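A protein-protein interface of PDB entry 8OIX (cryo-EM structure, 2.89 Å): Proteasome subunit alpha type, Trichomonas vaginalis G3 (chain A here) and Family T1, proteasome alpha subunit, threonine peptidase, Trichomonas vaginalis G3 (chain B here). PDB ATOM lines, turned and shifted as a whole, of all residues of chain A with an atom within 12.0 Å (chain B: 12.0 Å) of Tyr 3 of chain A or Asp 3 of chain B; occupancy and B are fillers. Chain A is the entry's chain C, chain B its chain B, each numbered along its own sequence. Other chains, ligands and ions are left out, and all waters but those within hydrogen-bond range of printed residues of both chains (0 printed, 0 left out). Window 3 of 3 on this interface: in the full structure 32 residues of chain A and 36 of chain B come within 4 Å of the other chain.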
ATOM      1  N   THR A   2     -13.582 -33.063   9.406  1.00  0.00           N
ATOM      2  CA  THR A   2     -14.689 -32.233   8.945  1.00  0.00           C
ATOM      3  C   THR A   2     -14.296 -31.411   7.723  1.00  0.00           C
ATOM      4  O   THR A   2     -13.238 -31.630   7.132  1.00  0.00           O
ATOM      5  CB  THR A   2     -15.185 -31.286  10.050  1.00  0.00           C
ATOM      6  OG1 THR A   2     -14.171 -30.315  10.345  1.00  0.00           O
ATOM      7  CG2 THR A   2     -15.517 -32.067  11.309  1.00  0.00           C
ATOM      8  N   TYR A   3     -15.172 -30.477   7.348  1.00  0.00           N
ATOM      9  CA  TYR A   3     -14.999 -29.602   6.190  1.00  0.00           C
ATOM     10  C   TYR A   3     -14.969 -30.375   4.877  1.00  0.00           C
ATOM     11  O   TYR A   3     -14.550 -29.838   3.847  1.00  0.00           O
ATOM     12  CB  TYR A   3     -13.740 -28.735   6.314  1.00  0.00           C
ATOM     13  CG  TYR A   3     -13.770 -27.783   7.484  1.00  0.00           C
ATOM     14  CD1 TYR A   3     -14.725 -26.780   7.561  1.00  0.00           C
ATOM     15  CD2 TYR A   3     -12.835 -27.879   8.505  1.00  0.00           C
ATOM     16  CE1 TYR A   3     -14.755 -25.907   8.625  1.00  0.00           C
ATOM     17  CE2 TYR A   3     -12.856 -27.007   9.573  1.00  0.00           C
ATOM     18  CZ  TYR A   3     -13.819 -26.025   9.628  1.00  0.00           C
ATOM     19  OH  TYR A   3     -13.847 -25.153  10.688  1.00  0.00           O
ATOM     20  N   ARG A   4     -15.402 -31.639   4.894  1.00  0.00           N
ATOM     21  CA  ARG A   4     -15.470 -32.409   3.658  1.00  0.00           C
ATOM     22  C   ARG A   4     -16.465 -31.795   2.682  1.00  0.00           C
ATOM     23  O   ARG A   4     -16.208 -31.739   1.474  1.00  0.00           O
ATOM     24  CB  ARG A   4     -15.839 -33.862   3.958  1.00  0.00           C
ATOM     25  CG  ARG A   4     -15.772 -34.769   2.741  1.00  0.00           C
ATOM     26  CD  ARG A   4     -16.170 -36.197   3.074  1.00  0.00           C
ATOM     27  NE  ARG A   4     -15.084 -36.931   3.714  1.00  0.00           N
ATOM     28  CZ  ARG A   4     -14.995 -38.254   3.752  1.00  0.00           C
ATOM     29  NH1 ARG A   4     -15.917 -39.026   3.203  1.00  0.00           N
ATOM     30  NH2 ARG A   4     -13.953 -38.815   4.360  1.00  0.00           N
ATOM     31  N   TYR A   5     -17.605 -31.326   3.189  1.00  0.00           N
ATOM     32  CA  TYR A   5     -18.650 -30.741   2.360  1.00  0.00           C
ATOM     33  C   TYR A   5     -18.632 -29.218   2.403  1.00  0.00           C
ATOM     34  O   TYR A   5     -19.659 -28.575   2.162  1.00  0.00           O
ATOM     35  CB  TYR A   5     -20.012 -31.280   2.794  1.00  0.00           C
ATOM     36  CG  TYR A   5     -20.003 -32.778   2.965  1.00  0.00           C
ATOM     37  CD1 TYR A   5     -19.747 -33.616   1.890  1.00  0.00           C
ATOM     38  CD2 TYR A   5     -20.218 -33.352   4.208  1.00  0.00           C
ATOM     39  CE1 TYR A   5     -19.723 -34.987   2.046  1.00  0.00           C
ATOM     40  CE2 TYR A   5     -20.196 -34.719   4.374  1.00  0.00           C
ATOM     41  CZ  TYR A   5     -19.947 -35.532   3.291  1.00  0.00           C
ATOM     42  OH  TYR A   5     -19.923 -36.895   3.458  1.00  0.00           O
ATOM     43  N   ASP A   6     -17.479 -28.631   2.707  1.00  0.00           N
ATOM     44  CA  ASP A   6     -17.312 -27.188   2.683  1.00  0.00           C
ATOM     45  C   ASP A   6     -16.925 -26.747   1.278  1.00  0.00           C
ATOM     46  O   ASP A   6     -16.157 -27.426   0.591  1.00  0.00           O
ATOM     47  CB  ASP A   6     -16.251 -26.757   3.699  1.00  0.00           C
ATOM     48  CG  ASP A   6     -15.755 -25.346   3.466  1.00  0.00           C
ATOM     49  OD1 ASP A   6     -16.581 -24.412   3.476  1.00  0.00           O
ATOM     50  OD2 ASP A   6     -14.533 -25.170   3.280  1.00  0.00           O
ATOM     51  N   ALA A   7     -17.462 -25.608   0.854  1.00  0.00           N
ATOM     52  CA  ALA A   7     -17.241 -25.115  -0.497  1.00  0.00           C
ATOM     53  C   ALA A   7     -16.086 -24.130  -0.593  1.00  0.00           C
ATOM     54  O   ALA A   7     -15.784 -23.663  -1.695  1.00  0.00           O
ATOM     55  CB  ALA A   7     -18.517 -24.461  -1.035  1.00  0.00           C
ATOM     56  N   GLY A   8     -15.421 -23.827   0.519  1.00  0.00           N
ATOM     57  CA  GLY A   8     -14.365 -22.837   0.523  1.00  0.00           C
ATOM     58  C   GLY A   8     -14.815 -21.501  -0.025  1.00  0.00           C
ATOM     59  O   GLY A   8     -14.173 -20.937  -0.917  1.00  0.00           O
ATOM     60  N   THR A   9     -15.930 -20.989   0.501  1.00  0.00           N
ATOM     61  CA  THR A   9     -16.473 -19.728   0.009  1.00  0.00           C
ATOM     62  C   THR A   9     -15.507 -18.580   0.263  1.00  0.00           C
ATOM     63  O   THR A   9     -15.427 -17.636  -0.531  1.00  0.00           O
ATOM     64  CB  THR A   9     -17.822 -19.444   0.663  1.00  0.00           C
ATOM     65  OG1 THR A   9     -17.628 -19.173   2.055  1.00  0.00           O
ATOM     66  CG2 THR A   9     -18.735 -20.641   0.520  1.00  0.00           C
ATOM     67  N   THR A  10     -14.777 -18.634   1.373  1.00  0.00           N
ATOM     68  CA  THR A  10     -13.773 -17.631   1.717  1.00  0.00           C
ATOM     69  C   THR A  10     -12.372 -18.157   1.445  1.00  0.00           C
ATOM     70  O   THR A  10     -11.450 -17.965   2.242  1.00  0.00           O
ATOM     71  CB  THR A  10     -13.918 -17.206   3.174  1.00  0.00           C
ATOM     72  OG1 THR A  10     -13.828 -18.360   4.017  1.00  0.00           O
ATOM     73  CG2 THR A  10     -15.259 -16.530   3.395  1.00  0.00           C
ATOM     74  N   THR A  11     -12.200 -18.849   0.323  1.00  0.00           N
ATOM     75  CA  THR A  11     -10.926 -19.425  -0.069  1.00  0.00           C
ATOM     76  C   THR A  11     -10.601 -19.002  -1.495  1.00  0.00           C
ATOM     77  O   THR A  11     -11.491 -18.868  -2.340  1.00  0.00           O
ATOM     78  CB  THR A  11     -10.961 -20.958   0.037  1.00  0.00           C
ATOM     79  OG1 THR A  11     -11.422 -21.333   1.340  1.00  0.00           O
ATOM     80  CG2 THR A  11      -9.582 -21.554  -0.187  1.00  0.00           C
ATOM     81  N   TYR A 123     -14.347 -13.828   5.414  1.00  0.00           N
ATOM     82  CA  TYR A 123     -14.439 -14.401   6.746  1.00  0.00           C
ATOM     83  C   TYR A 123     -15.710 -15.227   6.860  1.00  0.00           C
ATOM     84  O   TYR A 123     -16.689 -15.004   6.146  1.00  0.00           O
ATOM     85  CB  TYR A 123     -14.429 -13.311   7.826  1.00  0.00           C
ATOM     86  CG  TYR A 123     -13.219 -12.406   7.777  1.00  0.00           C
ATOM     87  CD1 TYR A 123     -12.030 -12.769   8.394  1.00  0.00           C
ATOM     88  CD2 TYR A 123     -13.270 -11.187   7.116  1.00  0.00           C
ATOM     89  CE1 TYR A 123     -10.925 -11.943   8.352  1.00  0.00           C
ATOM     90  CE2 TYR A 123     -12.168 -10.357   7.068  1.00  0.00           C
ATOM     91  CZ  TYR A 123     -10.999 -10.738   7.687  1.00  0.00           C
ATOM     92  OH  TYR A 123      -9.901  -9.912   7.642  1.00  0.00           O
ATOM     93  N   GLY A 124     -15.674 -16.200   7.768  1.00  0.00           N
ATOM     94  CA  GLY A 124     -16.862 -16.905   8.191  1.00  0.00           C
ATOM     95  C   GLY A 124     -17.274 -18.070   7.322  1.00  0.00           C
ATOM     96  O   GLY A 124     -18.190 -18.811   7.705  1.00  0.00           O
ATOM     97  N   GLY A 125     -16.635 -18.263   6.169  1.00  0.00           N
ATOM     98  CA  GLY A 125     -16.979 -19.380   5.305  1.00  0.00           C
ATOM     99  C   GLY A 125     -18.427 -19.414   4.880  1.00  0.00           C
ATOM    100  O   GLY A 125     -18.951 -20.490   4.574  1.00  0.00           O
ATOM    101  N   LEU A 126     -19.089 -18.265   4.844  1.00  0.00           N
ATOM    102  CA  LEU A 126     -20.487 -18.179   4.455  1.00  0.00           C
ATOM    103  C   LEU A 126     -20.602 -17.853   2.972  1.00  0.00           C
ATOM    104  O   LEU A 126     -19.638 -17.460   2.314  1.00  0.00           O
ATOM    105  CB  LEU A 126     -21.215 -17.123   5.288  1.00  0.00           C
ATOM    106  CG  LEU A 126     -21.268 -17.354   6.797  1.00  0.00           C
ATOM    107  CD1 LEU A 126     -22.124 -16.292   7.466  1.00  0.00           C
ATOM    108  CD2 LEU A 126     -21.801 -18.737   7.093  1.00  0.00           C
ATOM    109  N   ASP B   3     -16.997 -27.968  13.749  1.00  0.00           N
ATOM    110  CA  ASP B   3     -17.289 -26.684  13.122  1.00  0.00           C
ATOM    111  C   ASP B   3     -17.996 -26.885  11.788  1.00  0.00           C
ATOM    112  O   ASP B   3     -17.392 -27.331  10.813  1.00  0.00           O
ATOM    113  CB  ASP B   3     -16.005 -25.877  12.921  1.00  0.00           C
ATOM    114  CG  ASP B   3     -16.268 -24.460  12.451  1.00  0.00           C
ATOM    115  OD1 ASP B   3     -17.448 -24.058  12.370  1.00  0.00           O
ATOM    116  OD2 ASP B   3     -15.288 -23.747  12.158  1.00  0.00           O
ATOM    117  N   SER B   4     -19.284 -26.549  11.755  1.00  0.00           N
ATOM    118  CA  SER B   4     -20.086 -26.639  10.543  1.00  0.00           C
ATOM    119  C   SER B   4     -20.564 -25.268  10.079  1.00  0.00           C
ATOM    120  O   SER B   4     -21.512 -25.178   9.295  1.00  0.00           O
ATOM    121  CB  SER B   4     -21.279 -27.573  10.754  1.00  0.00           C
ATOM    122  OG  SER B   4     -21.822 -27.981   9.512  1.00  0.00           O
ATOM    123  N   ASP B   5     -19.916 -24.199  10.542  1.00  0.00           N
ATOM    124  CA  ASP B   5     -20.351 -22.838  10.253  1.00  0.00           C
ATOM    125  C   ASP B   5     -20.201 -22.467   8.780  1.00  0.00           C
ATOM    126  O   ASP B   5     -20.548 -21.343   8.405  1.00  0.00           O
ATOM    127  CB  ASP B   5     -19.569 -21.854  11.128  1.00  0.00           C
ATOM    128  CG  ASP B   5     -20.245 -20.498  11.241  1.00  0.00           C
ATOM    129  OD1 ASP B   5     -21.390 -20.353  10.766  1.00  0.00           O
ATOM    130  OD2 ASP B   5     -19.629 -19.573  11.812  1.00  0.00           O
ATOM    131  N   PHE B   6     -19.696 -23.364   7.938  1.00  0.00           N
ATOM    132  CA  PHE B   6     -19.630 -23.092   6.513  1.00  0.00           C
ATOM    133  C   PHE B   6     -21.010 -23.216   5.881  1.00  0.00           C
ATOM    134  O   PHE B   6     -21.855 -23.997   6.325  1.00  0.00           O
ATOM    135  CB  PHE B   6     -18.651 -24.044   5.825  1.00  0.00           C
ATOM    136  CG  PHE B   6     -18.955 -25.499   6.040  1.00  0.00           C
ATOM    137  CD1 PHE B   6     -19.867 -26.162   5.238  1.00  0.00           C
ATOM    138  CD2 PHE B   6     -18.318 -26.207   7.043  1.00  0.00           C
ATOM    139  CE1 PHE B   6     -20.144 -27.498   5.436  1.00  0.00           C
ATOM    140  CE2 PHE B   6     -18.588 -27.544   7.246  1.00  0.00           C
ATOM    141  CZ  PHE B   6     -19.502 -28.191   6.441  1.00  0.00           C
ATOM    142  N   SER B   7     -21.218 -22.457   4.810  1.00  0.00           N
ATOM    143  CA  SER B   7     -22.507 -22.426   4.134  1.00  0.00           C
ATOM    144  C   SER B   7     -22.643 -23.644   3.232  1.00  0.00           C
ATOM    145  O   SER B   7     -21.804 -23.872   2.355  1.00  0.00           O
ATOM    146  CB  SER B   7     -22.652 -21.137   3.330  1.00  0.00           C
ATOM    147  OG  SER B   7     -23.921 -21.064   2.708  1.00  0.00           O
ATOM    148  N   LEU B   8     -23.689 -24.438   3.459  1.00  0.00           N
ATOM    149  CA  LEU B   8     -23.986 -25.562   2.582  1.00  0.00           C
ATOM    150  C   LEU B   8     -24.776 -25.146   1.353  1.00  0.00           C
ATOM    151  O   LEU B   8     -24.849 -25.915   0.388  1.00  0.00           O
ATOM    152  CB  LEU B   8     -24.751 -26.639   3.350  1.00  0.00           C
ATOM    153  CG  LEU B   8     -23.999 -27.204   4.552  1.00  0.00           C
ATOM    154  CD1 LEU B   8     -24.525 -26.592   5.834  1.00  0.00           C
ATOM    155  CD2 LEU B   8     -24.106 -28.716   4.587  1.00  0.00           C
ATOM    156  N   THR B  10     -24.342 -22.872  -1.578  1.00  0.00           N
ATOM    157  CA  THR B  10     -23.289 -22.121  -2.241  1.00  0.00           C
ATOM    158  C   THR B  10     -23.552 -22.087  -3.736  1.00  0.00           C
ATOM    159  O   THR B  10     -24.202 -22.977  -4.290  1.00  0.00           O
ATOM    160  CB  THR B  10     -21.903 -22.721  -1.977  1.00  0.00           C
ATOM    161  OG1 THR B  10     -21.899 -24.103  -2.352  1.00  0.00           O
ATOM    162  CG2 THR B  10     -21.542 -22.594  -0.513  1.00  0.00           C
ATOM    163  N   GLN B 121     -28.008 -18.549   3.858  1.00  0.00           N
ATOM    164  CA  GLN B 121     -26.668 -17.982   3.887  1.00  0.00           C
ATOM    165  C   GLN B 121     -25.840 -18.460   5.069  1.00  0.00           C
ATOM    166  O   GLN B 121     -24.668 -18.804   4.892  1.00  0.00           O
ATOM    167  CB  GLN B 121     -26.745 -16.451   3.885  1.00  0.00           C
ATOM    168  CG  GLN B 121     -25.445 -15.783   3.490  1.00  0.00           C
ATOM    169  CD  GLN B 121     -25.670 -14.467   2.787  1.00  0.00           C
ATOM    170  OE1 GLN B 121     -26.746 -13.880   2.878  1.00  0.00           O
ATOM    171  NE2 GLN B 121     -24.656 -13.996   2.072  1.00  0.00           N
ATOM    172  N   ILE B 122     -26.406 -18.484   6.280  1.00  0.00           N
ATOM    173  CA  ILE B 122     -25.622 -18.917   7.432  1.00  0.00           C
ATOM    174  C   ILE B 122     -25.238 -20.385   7.271  1.00  0.00           C
ATOM    175  O   ILE B 122     -25.817 -21.131   6.471  1.00  0.00           O
ATOM    176  CB  ILE B 122     -26.354 -18.697   8.765  1.00  0.00           C
ATOM    177  CG1 ILE B 122     -27.708 -19.404   8.768  1.00  0.00           C
ATOM    178  CG2 ILE B 122     -26.509 -17.217   9.037  1.00  0.00           C
ATOM    179  CD1 ILE B 122     -28.062 -20.026  10.098  1.00  0.00           C
ATOM    180  N   GLY B 123     -24.244 -20.799   8.046  1.00  0.00           N
ATOM    181  CA  GLY B 123     -23.674 -22.117   7.913  1.00  0.00           C
ATOM    182  C   GLY B 123     -24.301 -23.127   8.854  1.00  0.00           C
ATOM    183  O   GLY B 123     -24.934 -22.775   9.847  1.00  0.00           O
ATOM    184  N   GLY B 124     -24.113 -24.400   8.522  1.00  0.00           N
ATOM    185  CA  GLY B 124     -24.629 -25.482   9.326  1.00  0.00           C
ATOM    186  C   GLY B 124     -26.099 -25.773   9.140  1.00  0.00           C
ATOM    187  O   GLY B 124     -26.632 -26.640   9.842  1.00  0.00           O
ATOM    188  N   VAL B 125     -26.771 -25.086   8.218  1.00  0.00           N
ATOM    189  CA  VAL B 125     -28.200 -25.250   8.003  1.00  0.00           C
ATOM    190  C   VAL B 125     -28.468 -25.415   6.516  1.00  0.00           C
ATOM    191  O   VAL B 125     -27.646 -25.070   5.665  1.00  0.00           O
ATOM    192  CB  VAL B 125     -29.018 -24.060   8.550  1.00  0.00           C
ATOM    193  CG1 VAL B 125     -28.828 -23.917  10.043  1.00  0.00           C
ATOM    194  CG2 VAL B 125     -28.624 -22.786   7.837  1.00  0.00           C
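OH of Tyr 3 of chain A is in hydrogen-bond range of OD2 of Asp 3 of chain B (2.5 Å).
The backbone NH (N) of Ser 7 of chain B lies within hydrogen-bond range of the backbone carbonyl oxygen (O) of Gly 125 of chain A, at 3.0 Å.
The backbone NH (N) of Asp 5 of chain B is in hydrogen-bond range of the side-chain carboxylate (OD1) of Asp 3 of chain B (3.1 Å).
The side-chain hydroxyl (OG) of Ser 7 of chain B lies within hydrogen-bond range of the backbone carbonyl oxygen (O) of Gln 121 of chain B, 3.2 Å away.
The backbone NH (N) of Gly 124 of chain B lies within hydrogen-bond range of the backbone carbonyl oxygen (O) of Phe 6 of chain B, at 3.2 Å.
The backbone carbonyl oxygen (O) of Leu 126 of chain A is in hydrogen-bond range of the side-chain hydroxyl (OG1) of Thr 9 of chain A (2.7 Å).
The backbone carbonyl oxygen of Gly 125 of chain A lies close to the side-chain hydroxyl of Thr 9 of chain A (3.1 Å).
The side-chain carboxylate (OD2) of Asp 6 of chain A lies within hydrogen-bond range of the backbone NH (N) of Gly 8 of chain A.
Phe 6 of chain B touches Tyr 3 of chain A.
CE1 of Phe 6 of chain B touches O of Tyr 5 of chain A (3.5 Å).
Asp 6 of chain A touches Phe 6 of chain B (OD1 to CB, 3.2 Å).
Thr 10 of chain B touches Ala 7 of chain A (CG2 to CB, 3.6 Å).
Thr 10 of chain B touches Thr 9 of chain A (CG2 to CG2, 3.6 Å).
O of Gly 125 of chain A touches CA of Phe 6 of chain B, at 3.3 Å.
Leu 126 of chain A touches Asp 5 of chain B.
Leu 126 of chain A touches Ser 7 of chain B.
CD2 of Leu 126 of chain A touches O of Gln 121 of chain B (3.6 Å).
Gly 123 of chain B touches Leu 126 of chain A.
No residue of chain B comes within 4 Å of Thr 2 of chain A.
Printed residues of chain B within 4 Å of Tyr 3 of chain A: Asp 3 and Phe 6.
Arg 4 of chain A touches none of the printed residues of chain B.
Of the printed residues of chain B, Asp 6 of chain A touches Phe 6.
Of the printed residues of chain B, Ala 7 of chain A touches Thr 10 (3.6 Å).
Of the printed residues of chain B, Thr 9 of chain A touches Thr 10.
Of the printed residues of chain B, Gly 124 of chain A touches Asp 5 (3.5 Å).
Printed residues of chain B within 4 Å of Gly 125 of chain A: Phe 6 (3.3 Å) and Ser 7 (3.0 Å).
Of chain A, only Tyr 3 (2.5 Å) comes within 4 Å of Asp 3 of chain B.
No residue of chain A comes within 4 Å of Ser 4 of chain B.
Leu 8 of chain B touches none of the printed residues of chain A.
Of the printed residues of chain A, Thr 10 of chain B touches Ala 7 and Thr 9.
The nearest printed residue of chain A that does not touch Ile 122 of chain B is Gly 125 of chain A (6.8 Å).
Printed residues of chain A that touch a printed residue of chain B: Tyr 3, Tyr 5, Asp 6, Ala 7, Thr 9, Gly 124, Gly 125 and Leu 126.
Hydrophobic or aromatic side chains of chain A that line the printed part of chain B: Tyr 3, Ala 7 and Leu 126.
Among the printed residues, 14 pairs touch across the chains.
Among the printed residues, no Asp or Glu carboxylate lies within 4 Å of a Lys or Arg side-chain nitrogen of the other chain.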
